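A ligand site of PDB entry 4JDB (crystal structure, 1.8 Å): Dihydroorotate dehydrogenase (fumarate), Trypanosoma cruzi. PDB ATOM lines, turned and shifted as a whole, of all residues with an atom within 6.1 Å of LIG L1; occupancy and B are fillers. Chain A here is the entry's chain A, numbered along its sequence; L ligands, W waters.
Water W1 lies within hydrogen-bond range of O1 of LIG L1 (2.9 Å) and OD1 of Asn 68 (3.0 Å).
The side-chain amino group of Lys 44 lies within hydrogen-bond range of an oxygen (O2) of LG2 L2 (2.8 Å). O1 of LG2 L2 lies within hydrogen-bond range of ND2 of Asn 195 (3.2 Å). The backbone NH of Leu 72 lies within hydrogen-bond range of an oxygen (O2) of LIG L1, 2.9 Å away. O4 of LIG L1 sits at hydrogen-bond distance from ND2 of Asn 128, 2.9 Å away. An oxygen (O2) of LIG L1 lies within salt-bridge range of the side-chain amino group (NZ) of Lys 44 (3.0 Å). O1 of LIG L1 sits at hydrogen-bond distance from N of Gly 71, at 3.0 Å. The side-chain hydroxyl (OG) of Ser 196 sits at hydrogen-bond distance from an oxygen (O3) of LIG L1, at 2.8 Å. The backbone NH (N) of Met 70 lies within hydrogen-bond range of an oxygen (O1) of LIG L1 (3.1 Å). The side-chain amide nitrogen (ND2) of Asn 68 sits at hydrogen-bond distance from an oxygen (O3) of LIG L1, 2.9 Å away. The backbone NH (N) of Ala 20 lies within hydrogen-bond range of an oxygen (O3) of LG2 L2 (3.5 Å). The side-chain amide nitrogen (ND2) of Asn 128 lies within hydrogen-bond range of an oxygen (O1) of LG2 L2, 3.3 Å away. NH2 of Arg 51 is in hydrogen-bond range of O5 of LIG L1 (3.4 Å). The side-chain amino group (NZ) of Lys 165 lies within hydrogen-bond range of an oxygen (O3) of LG2 L2, 2.9 Å away. O3 of LG2 L2 lies within hydrogen-bond range of O of Ala 20, at 2.8 Å. The side-chain amide oxygen of Asn 195 is in hydrogen-bond range of a nitrogen (N2) of LIG L1. OG of Ser 45 is in hydrogen-bond range of N2 of LG2 L2 (2.8 Å).
ND2 of Asn 128 lies within hydrogen-bond range of OG of Ser 45, 3.5 Å away. The backbone carbonyl oxygen of Ser 69 sits at hydrogen-bond distance from the side-chain amide nitrogen of Asn 54, 2.8 Å away. The side-chain amide oxygen of Asn 68 lies within hydrogen-bond range of the backbone NH of Met 70 (3.2 Å). OD1 of Asn 128 lies within hydrogen-bond range of N of Ser 130 (2.9 Å). The backbone carbonyl oxygen (O) of Leu 72 sits at hydrogen-bond distance from the guanidinium group (NE) of Arg 51 (3.4 Å). The backbone carbonyl oxygen (O) of Asn 128 is in hydrogen-bond range of the side-chain sulfur (SG) of Cys 131 (3.1 Å). The backbone carbonyl oxygen (O) of Asn 68 is in hydrogen-bond range of the backbone NH (N) of Gly 220 (2.8 Å). The side-chain amide oxygen (OD1) of Asn 128 is in hydrogen-bond range of the side-chain amide nitrogen (ND2) of Asn 195 (3.4 Å).
A nitrogen (N2) of LIG L1 sits close to a nitrogen (N1) of LG2 L2.
ND2 of Asn 54 touches C14 of LIG L1 (3.9 Å). C of Ser 69 touches O1 of LIG L1 (3.97 Å). Hydrophobic or aromatic side chains within 4 Å of LIG L1: Met 70 and Leu 72. Of the 22 residues printed, 11 come within 4 Å of LIG L1. Along chain A the residues within 4 Å of LIG L1 span positions 44 to 196. The nearest printed residue that does not touch LIG L1 is Pro 73 (4.03 Å).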
ATOM      1  N   ALA A  20     -24.397 -19.861  -6.888  1.00  0.00           N
ATOM      2  CA  ALA A  20     -24.957 -20.027  -8.178  1.00  0.00           C
ATOM      3  C   ALA A  20     -26.471 -20.264  -8.174  1.00  0.00           C
ATOM      4  O   ALA A  20     -26.979 -21.007  -7.316  1.00  0.00           O
ATOM      5  CB  ALA A  20     -24.222 -21.195  -8.948  1.00  0.00           C
ATOM      6  N   LYS A  44     -25.748 -18.012 -13.290  1.00  0.00           N
ATOM      7  CA  LYS A  44     -26.566 -19.173 -13.205  1.00  0.00           C
ATOM      8  C   LYS A  44     -25.939 -20.337 -13.979  1.00  0.00           C
ATOM      9  O   LYS A  44     -25.508 -20.110 -15.109  1.00  0.00           O
ATOM     10  CB  LYS A  44     -27.885 -18.883 -13.857  1.00  0.00           C
ATOM     11  CG  LYS A  44     -28.848 -20.037 -14.027  1.00  0.00           C
ATOM     12  CD  LYS A  44     -29.258 -20.731 -12.785  1.00  0.00           C
ATOM     13  CE  LYS A  44     -30.067 -22.029 -13.037  1.00  0.00           C
ATOM     14  NZ  LYS A  44     -30.545 -22.670 -11.767  1.00  0.00           N
ATOM     15  N   SER A  45     -25.953 -21.531 -13.396  1.00  0.00           N
ATOM     16  CA  SER A  45     -25.465 -22.777 -14.076  1.00  0.00           C
ATOM     17  C   SER A  45     -26.198 -22.836 -15.412  1.00  0.00           C
ATOM     18  O   SER A  45     -27.390 -22.784 -15.462  1.00  0.00           O
ATOM     19  CB  SER A  45     -25.734 -23.965 -13.250  1.00  0.00           C
ATOM     20  OG  SER A  45     -24.844 -24.009 -12.197  1.00  0.00           O
ATOM     21  N   ARG A  51     -33.182 -22.805 -21.421  1.00  0.00           N
ATOM     22  CA  ARG A  51     -34.146 -23.653 -20.800  1.00  0.00           C
ATOM     23  C   ARG A  51     -35.143 -22.833 -20.038  1.00  0.00           C
ATOM     24  O   ARG A  51     -34.770 -21.890 -19.383  1.00  0.00           O
ATOM     25  CB  ARG A  51     -33.539 -24.644 -19.820  1.00  0.00           C
ATOM     26  CG  ARG A  51     -32.676 -25.734 -20.428  1.00  0.00           C
ATOM     27  CD  ARG A  51     -32.027 -26.551 -19.367  1.00  0.00           C
ATOM     28  NE  ARG A  51     -32.889 -27.195 -18.353  1.00  0.00           N
ATOM     29  CZ  ARG A  51     -33.531 -28.365 -18.486  1.00  0.00           C
ATOM     30  NH1 ARG A  51     -33.424 -29.105 -19.595  1.00  0.00           N
ATOM     31  NH2 ARG A  51     -34.233 -28.819 -17.499  1.00  0.00           N
ATOM     32  N   ASN A  54     -38.396 -26.021 -14.722  1.00  0.00           N
ATOM     33  CA  ASN A  54     -39.534 -26.778 -14.254  1.00  0.00           C
ATOM     34  C   ASN A  54     -40.795 -25.913 -14.083  1.00  0.00           C
ATOM     35  O   ASN A  54     -40.685 -24.685 -13.985  1.00  0.00           O
ATOM     36  CB  ASN A  54     -39.153 -27.475 -12.934  1.00  0.00           C
ATOM     37  CG  ASN A  54     -38.304 -28.704 -13.098  1.00  0.00           C
ATOM     38  OD1 ASN A  54     -38.157 -29.232 -14.199  1.00  0.00           O
ATOM     39  ND2 ASN A  54     -37.642 -29.102 -12.040  1.00  0.00           N
ATOM     40  N   ASN A  68     -36.141 -26.061  -3.497  1.00  0.00           N
ATOM     41  CA  ASN A  68     -36.318 -25.744  -4.852  1.00  0.00           C
ATOM     42  C   ASN A  68     -36.138 -26.962  -5.761  1.00  0.00           C
ATOM     43  O   ASN A  68     -35.334 -27.879  -5.469  1.00  0.00           O
ATOM     44  CB  ASN A  68     -35.323 -24.604  -5.323  1.00  0.00           C
ATOM     45  CG  ASN A  68     -33.972 -25.145  -5.774  1.00  0.00           C
ATOM     46  OD1 ASN A  68     -33.793 -25.608  -6.944  1.00  0.00           O
ATOM     47  ND2 ASN A  68     -33.028 -25.128  -4.882  1.00  0.00           N
ATOM     48  N   SER A  69     -36.844 -26.905  -6.853  1.00  0.00           N
ATOM     49  CA  SER A  69     -36.540 -27.769  -7.989  1.00  0.00           C
ATOM     50  C   SER A  69     -36.686 -26.918  -9.236  1.00  0.00           C
ATOM     51  O   SER A  69     -37.638 -27.082 -10.058  1.00  0.00           O
ATOM     52  CB  SER A  69     -37.419 -28.986  -7.976  1.00  0.00           C
ATOM     53  OG  SER A  69     -37.054 -29.829  -9.080  1.00  0.00           O
ATOM     54  N   MET A  70     -35.761 -26.018  -9.383  1.00  0.00           N
ATOM     55  CA  MET A  70     -35.872 -25.037 -10.475  1.00  0.00           C
ATOM     56  C   MET A  70     -35.800 -25.723 -11.867  1.00  0.00           C
ATOM     57  O   MET A  70     -36.504 -25.384 -12.834  1.00  0.00           O
ATOM     58  CB  MET A  70     -34.811 -24.054 -10.387  1.00  0.00           C
ATOM     59  CG  MET A  70     -34.659 -23.244  -9.127  1.00  0.00           C
ATOM     60  SD  MET A  70     -36.065 -22.268  -8.692  1.00  0.00           S
ATOM     61  CE  MET A  70     -36.080 -21.029  -9.967  1.00  0.00           C
ATOM     62  N   GLY A  71     -34.947 -26.740 -11.974  1.00  0.00           N
ATOM     63  CA  GLY A  71     -34.754 -27.412 -13.249  1.00  0.00           C
ATOM     64  C   GLY A  71     -33.844 -26.746 -14.261  1.00  0.00           C
ATOM     65  O   GLY A  71     -34.115 -26.823 -15.462  1.00  0.00           O
ATOM     66  N   LEU A  72     -32.837 -26.035 -13.794  1.00  0.00           N
ATOM     67  CA  LEU A  72     -31.930 -25.309 -14.616  1.00  0.00           C
ATOM     68  C   LEU A  72     -32.540 -24.364 -15.626  1.00  0.00           C
ATOM     69  O   LEU A  72     -32.136 -24.325 -16.789  1.00  0.00           O
ATOM     70  CB  LEU A  72     -31.049 -26.331 -15.397  1.00  0.00           C
ATOM     71  CG  LEU A  72     -29.764 -26.790 -14.791  1.00  0.00           C
ATOM     72  CD1 LEU A  72     -29.149 -27.889 -15.682  1.00  0.00           C
ATOM     73  CD2 LEU A  72     -28.755 -25.775 -14.341  1.00  0.00           C
ATOM     74  N   PRO A  73     -33.464 -23.530 -15.219  1.00  0.00           N
ATOM     75  CA  PRO A  73     -33.853 -22.438 -16.137  1.00  0.00           C
ATOM     76  C   PRO A  73     -32.670 -21.500 -16.384  1.00  0.00           C
ATOM     77  O   PRO A  73     -32.037 -21.020 -15.443  1.00  0.00           O
ATOM     78  CB  PRO A  73     -34.937 -21.705 -15.366  1.00  0.00           C
ATOM     79  CG  PRO A  73     -34.651 -21.964 -13.908  1.00  0.00           C
ATOM     80  CD  PRO A  73     -33.806 -23.255 -13.806  1.00  0.00           C
ATOM     81  N   SER A 100     -23.417 -26.360 -16.179  1.00  0.00           N
ATOM     82  CA  SER A 100     -24.071 -27.528 -15.751  1.00  0.00           C
ATOM     83  C   SER A 100     -24.687 -28.282 -16.889  1.00  0.00           C
ATOM     84  O   SER A 100     -25.876 -28.537 -16.915  1.00  0.00           O
ATOM     85  CB  SER A 100     -25.163 -27.186 -14.718  1.00  0.00           C
ATOM     86  OG  SER A 100     -25.740 -28.360 -14.229  1.00  0.00           O
ATOM     87  N   LEU A 102     -25.860 -31.390 -19.271  1.00  0.00           N
ATOM     88  CA  LEU A 102     -26.673 -32.560 -18.967  1.00  0.00           C
ATOM     89  C   LEU A 102     -25.982 -33.843 -19.403  1.00  0.00           C
ATOM     90  O   LEU A 102     -26.475 -34.975 -19.139  1.00  0.00           O
ATOM     91  CB  LEU A 102     -28.060 -32.495 -19.628  1.00  0.00           C
ATOM     92  CG  LEU A 102     -28.939 -31.273 -19.271  1.00  0.00           C
ATOM     93  CD1 LEU A 102     -30.386 -31.531 -19.671  1.00  0.00           C
ATOM     94  CD2 LEU A 102     -28.857 -30.894 -17.826  1.00  0.00           C
ATOM     95  N   ASN A 128     -20.454 -27.409 -12.194  1.00  0.00           N
ATOM     96  CA  ASN A 128     -21.424 -27.928 -11.299  1.00  0.00           C
ATOM     97  C   ASN A 128     -21.580 -29.464 -11.404  1.00  0.00           C
ATOM     98  O   ASN A 128     -22.152 -29.981 -12.399  1.00  0.00           O
ATOM     99  CB  ASN A 128     -22.809 -27.333 -11.609  1.00  0.00           C
ATOM    100  CG  ASN A 128     -23.851 -27.754 -10.641  1.00  0.00           C
ATOM    101  OD1 ASN A 128     -23.603 -28.479  -9.685  1.00  0.00           O
ATOM    102  ND2 ASN A 128     -25.041 -27.197 -10.804  1.00  0.00           N
ATOM    103  N   SER A 130     -23.310 -31.349  -9.361  1.00  0.00           N
ATOM    104  CA  SER A 130     -24.733 -31.895  -9.416  1.00  0.00           C
ATOM    105  C   SER A 130     -25.457 -31.944 -10.779  1.00  0.00           C
ATOM    106  O   SER A 130     -26.623 -32.223 -10.829  1.00  0.00           O
ATOM    107  CB  SER A 130     -25.603 -31.159  -8.469  1.00  0.00           C
ATOM    108  OG  SER A 130     -24.962 -31.259  -7.176  1.00  0.00           O
ATOM    109  N   CYS A 131     -24.836 -31.634 -11.897  1.00  0.00           N
ATOM    110  CA  CYS A 131     -25.574 -31.774 -13.123  1.00  0.00           C
ATOM    111  C   CYS A 131     -26.278 -33.195 -13.003  1.00  0.00           C
ATOM    112  O   CYS A 131     -25.807 -34.169 -12.268  1.00  0.00           O
ATOM    113  CB  CYS A 131     -24.688 -31.598 -14.354  1.00  0.00           C
ATOM    114  SG  CYS A 131     -22.962 -32.252 -14.301  1.00  0.00           S
ATOM    115  N   PRO A 132     -27.480 -33.294 -13.587  1.00  0.00           N
ATOM    116  CA  PRO A 132     -28.112 -34.597 -13.528  1.00  0.00           C
ATOM    117  C   PRO A 132     -27.320 -35.470 -14.468  1.00  0.00           C
ATOM    118  O   PRO A 132     -26.638 -34.987 -15.342  1.00  0.00           O
ATOM    119  CB  PRO A 132     -29.539 -34.308 -14.048  1.00  0.00           C
ATOM    120  CG  PRO A 132     -29.320 -33.184 -15.005  1.00  0.00           C
ATOM    121  CD  PRO A 132     -28.245 -32.332 -14.413  1.00  0.00           C
ATOM    122  N   LYS A 165     -18.383 -27.291  -8.154  1.00  0.00           N
ATOM    123  CA  LYS A 165     -19.469 -27.226  -7.137  1.00  0.00           C
ATOM    124  C   LYS A 165     -19.959 -28.607  -6.724  1.00  0.00           C
ATOM    125  O   LYS A 165     -20.336 -29.420  -7.563  1.00  0.00           O
ATOM    126  CB  LYS A 165     -20.583 -26.347  -7.659  1.00  0.00           C
ATOM    127  CG  LYS A 165     -21.794 -26.273  -6.758  1.00  0.00           C
ATOM    128  CD  LYS A 165     -21.505 -25.242  -5.674  1.00  0.00           C
ATOM    129  CE  LYS A 165     -22.803 -24.850  -4.979  1.00  0.00           C
ATOM    130  NZ  LYS A 165     -23.668 -23.957  -5.794  1.00  0.00           N
ATOM    131  N   ASN A 195     -23.473 -27.565  -2.611  1.00  0.00           N
ATOM    132  CA  ASN A 195     -24.839 -27.450  -3.216  1.00  0.00           C
ATOM    133  C   ASN A 195     -25.980 -27.804  -2.206  1.00  0.00           C
ATOM    134  O   ASN A 195     -25.753 -28.147  -1.021  1.00  0.00           O
ATOM    135  CB  ASN A 195     -24.920 -28.305  -4.514  1.00  0.00           C
ATOM    136  CG  ASN A 195     -25.743 -27.639  -5.612  1.00  0.00           C
ATOM    137  OD1 ASN A 195     -26.919 -27.327  -5.405  1.00  0.00           O
ATOM    138  ND2 ASN A 195     -25.144 -27.457  -6.806  1.00  0.00           N
ATOM    139  N   SER A 196     -27.239 -27.720  -2.641  1.00  0.00           N
ATOM    140  CA  SER A 196     -28.368 -28.087  -1.770  1.00  0.00           C
ATOM    141  C   SER A 196     -28.340 -29.476  -1.255  1.00  0.00           C
ATOM    142  O   SER A 196     -27.723 -30.381  -1.844  1.00  0.00           O
ATOM    143  CB  SER A 196     -29.722 -27.812  -2.406  1.00  0.00           C
ATOM    144  OG  SER A 196     -29.718 -27.992  -3.739  1.00  0.00           O
ATOM    145  N   LYS A 215     -41.543 -32.965  -9.192  1.00  0.00           N
ATOM    146  CA  LYS A 215     -41.088 -34.072  -8.412  1.00  0.00           C
ATOM    147  C   LYS A 215     -41.912 -34.344  -7.134  1.00  0.00           C
ATOM    148  O   LYS A 215     -41.372 -34.766  -6.144  1.00  0.00           O
ATOM    149  CB  LYS A 215     -39.604 -33.832  -8.054  1.00  0.00           C
ATOM    150  CG  LYS A 215     -38.685 -33.645  -9.277  1.00  0.00           C
ATOM    151  CD  LYS A 215     -37.217 -33.480  -8.864  1.00  0.00           C
ATOM    152  CE  LYS A 215     -36.747 -34.390  -7.700  1.00  0.00           C
ATOM    153  NZ  LYS A 215     -35.286 -34.279  -7.493  1.00  0.00           N
ATOM    154  N   GLY A 220     -34.223 -29.569  -3.488  1.00  0.00           N
ATOM    155  CA  GLY A 220     -33.045 -29.356  -2.729  1.00  0.00           C
ATOM    156  C   GLY A 220     -33.246 -28.309  -1.649  1.00  0.00           C
ATOM    157  O   GLY A 220     -33.939 -27.329  -1.862  1.00  0.00           O
HETATM  158  O1  LIG L   1     -32.784 -26.746  -9.967  1.00  0.00           O
HETATM  159  C1  LIG L   1     -31.706 -26.190 -10.250  1.00  0.00           C
HETATM  160  O2  LIG L   1     -31.606 -25.471 -11.257  1.00  0.00           O
HETATM  161  C2  LIG L   1     -30.594 -26.336  -9.331  1.00  0.00           C
HETATM  162  N1  LIG L   1     -30.971 -26.117  -7.955  1.00  0.00           N
HETATM  163  C3  LIG L   1     -30.063 -26.283  -6.924  1.00  0.00           C
HETATM  164  O3  LIG L   1     -30.417 -26.138  -5.744  1.00  0.00           O
HETATM  165  N2  LIG L   1     -28.788 -26.662  -7.285  1.00  0.00           N
HETATM  166  C4  LIG L   1     -28.386 -26.979  -8.616  1.00  0.00           C
HETATM  167  O4  LIG L   1     -27.200 -27.339  -8.824  1.00  0.00           O
HETATM  168  C5  LIG L   1     -29.337 -26.776  -9.655  1.00  0.00           C
HETATM  169  C6  LIG L   1     -28.994 -27.068 -10.988  1.00  0.00           C
HETATM  170  C7  LIG L   1     -28.745 -28.603 -11.152  1.00  0.00           C
HETATM  171  C8  LIG L   1     -30.033 -29.218 -11.334  1.00  0.00           C
HETATM  172  C9  LIG L   1     -30.548 -29.555 -12.596  1.00  0.00           C
HETATM  173  C10 LIG L   1     -31.839 -30.120 -12.757  1.00  0.00           C
HETATM  174  C11 LIG L   1     -32.357 -30.470 -14.021  1.00  0.00           C
HETATM  175  C12 LIG L   1     -33.655 -31.021 -14.134  1.00  0.00           C
HETATM  176  O5  LIG L   1     -34.166 -31.387 -15.334  1.00  0.00           O
HETATM  177  C13 LIG L   1     -33.156 -31.942 -16.237  1.00  0.00           C
HETATM  178  C14 LIG L   1     -34.475 -31.212 -13.003  1.00  0.00           C
HETATM  179  C15 LIG L   1     -33.964 -30.888 -11.781  1.00  0.00           C
HETATM  180  C16 LIG L   1     -32.659 -30.332 -11.671  1.00  0.00           C
HETATM  181  C17 LIG L   1     -32.171 -30.025 -10.404  1.00  0.00           C
HETATM  182  C18 LIG L   1     -30.874 -29.480 -10.230  1.00  0.00           C
HETATM  183  N1  LG2 L   2     -26.355 -24.379  -7.434  1.00  0.00           N
HETATM  184  C1  LG2 L   2     -25.676 -24.448  -8.592  1.00  0.00           C
HETATM  185  O1  LG2 L   2     -24.501 -24.853  -8.484  1.00  0.00           O
HETATM  186  N2  LG2 L   2     -26.218 -24.088  -9.756  1.00  0.00           N
HETATM  187  C2  LG2 L   2     -27.433 -23.536  -9.854  1.00  0.00           C
HETATM  188  O2  LG2 L   2     -27.928 -23.121 -10.913  1.00  0.00           O
HETATM  189  C3  LG2 L   2     -28.234 -23.391  -8.662  1.00  0.00           C
HETATM  190  N3  LG2 L   2     -29.458 -22.871  -8.704  1.00  0.00           N
HETATM  191  C4  LG2 L   2     -30.104 -22.558  -7.531  1.00  0.00           C
HETATM  192  C5  LG2 L   2     -31.357 -21.894  -7.573  1.00  0.00           C
HETATM  193  C6  LG2 L   2     -32.024 -21.610  -6.373  1.00  0.00           C
HETATM  194  C7  LG2 L   2     -33.354 -20.882  -6.426  1.00  0.00           C
HETATM  195  C8  LG2 L   2     -31.387 -21.977  -5.098  1.00  0.00           C
HETATM  196  C9  LG2 L   2     -32.114 -21.757  -3.797  1.00  0.00           C
HETATM  197  C10 LG2 L   2     -30.163 -22.656  -5.094  1.00  0.00           C
HETATM  198  C11 LG2 L   2     -29.504 -22.928  -6.259  1.00  0.00           C
HETATM  199  N4  LG2 L   2     -28.250 -23.609  -6.250  1.00  0.00           N
HETATM  200  C12 LG2 L   2     -27.594 -23.791  -7.414  1.00  0.00           C
HETATM  201  C13 LG2 L   2     -27.631 -23.996  -5.033  1.00  0.00           C
HETATM  202  C14 LG2 L   2     -27.049 -22.805  -4.325  1.00  0.00           C
HETATM  203  O3  LG2 L   2     -26.008 -22.394  -5.096  1.00  0.00           O
HETATM  204  C15 LG2 L   2     -26.500 -23.190  -2.975  1.00  0.00           C
HETATM  205  O4  LG2 L   2     -25.508 -24.203  -3.233  1.00  0.00           O
HETATM  206  C16 LG2 L   2     -27.550 -23.717  -1.956  1.00  0.00           C
HETATM  207  O5  LG2 L   2     -28.815 -22.992  -2.053  1.00  0.00           O
HETATM  208  C17 LG2 L   2     -27.051 -23.597  -0.495  1.00  0.00           C
HETATM  209  O6  LG2 L   2     -26.653 -22.286  -0.097  1.00  0.00           O
HETATM  210  P1  LG2 L   2     -27.734 -21.571   0.903  1.00  0.00           P
HETATM  211  O7  LG2 L   2     -27.970 -22.484   2.070  1.00  0.00           O
HETATM  212  O8  LG2 L   2     -28.986 -21.507   0.040  1.00  0.00           O
HETATM  213  O9  LG2 L   2     -27.097 -20.219   0.999  1.00  0.00           O
HETATM  214  O   HOH W   1     -33.019 -28.388  -7.599  1.00  0.00           O
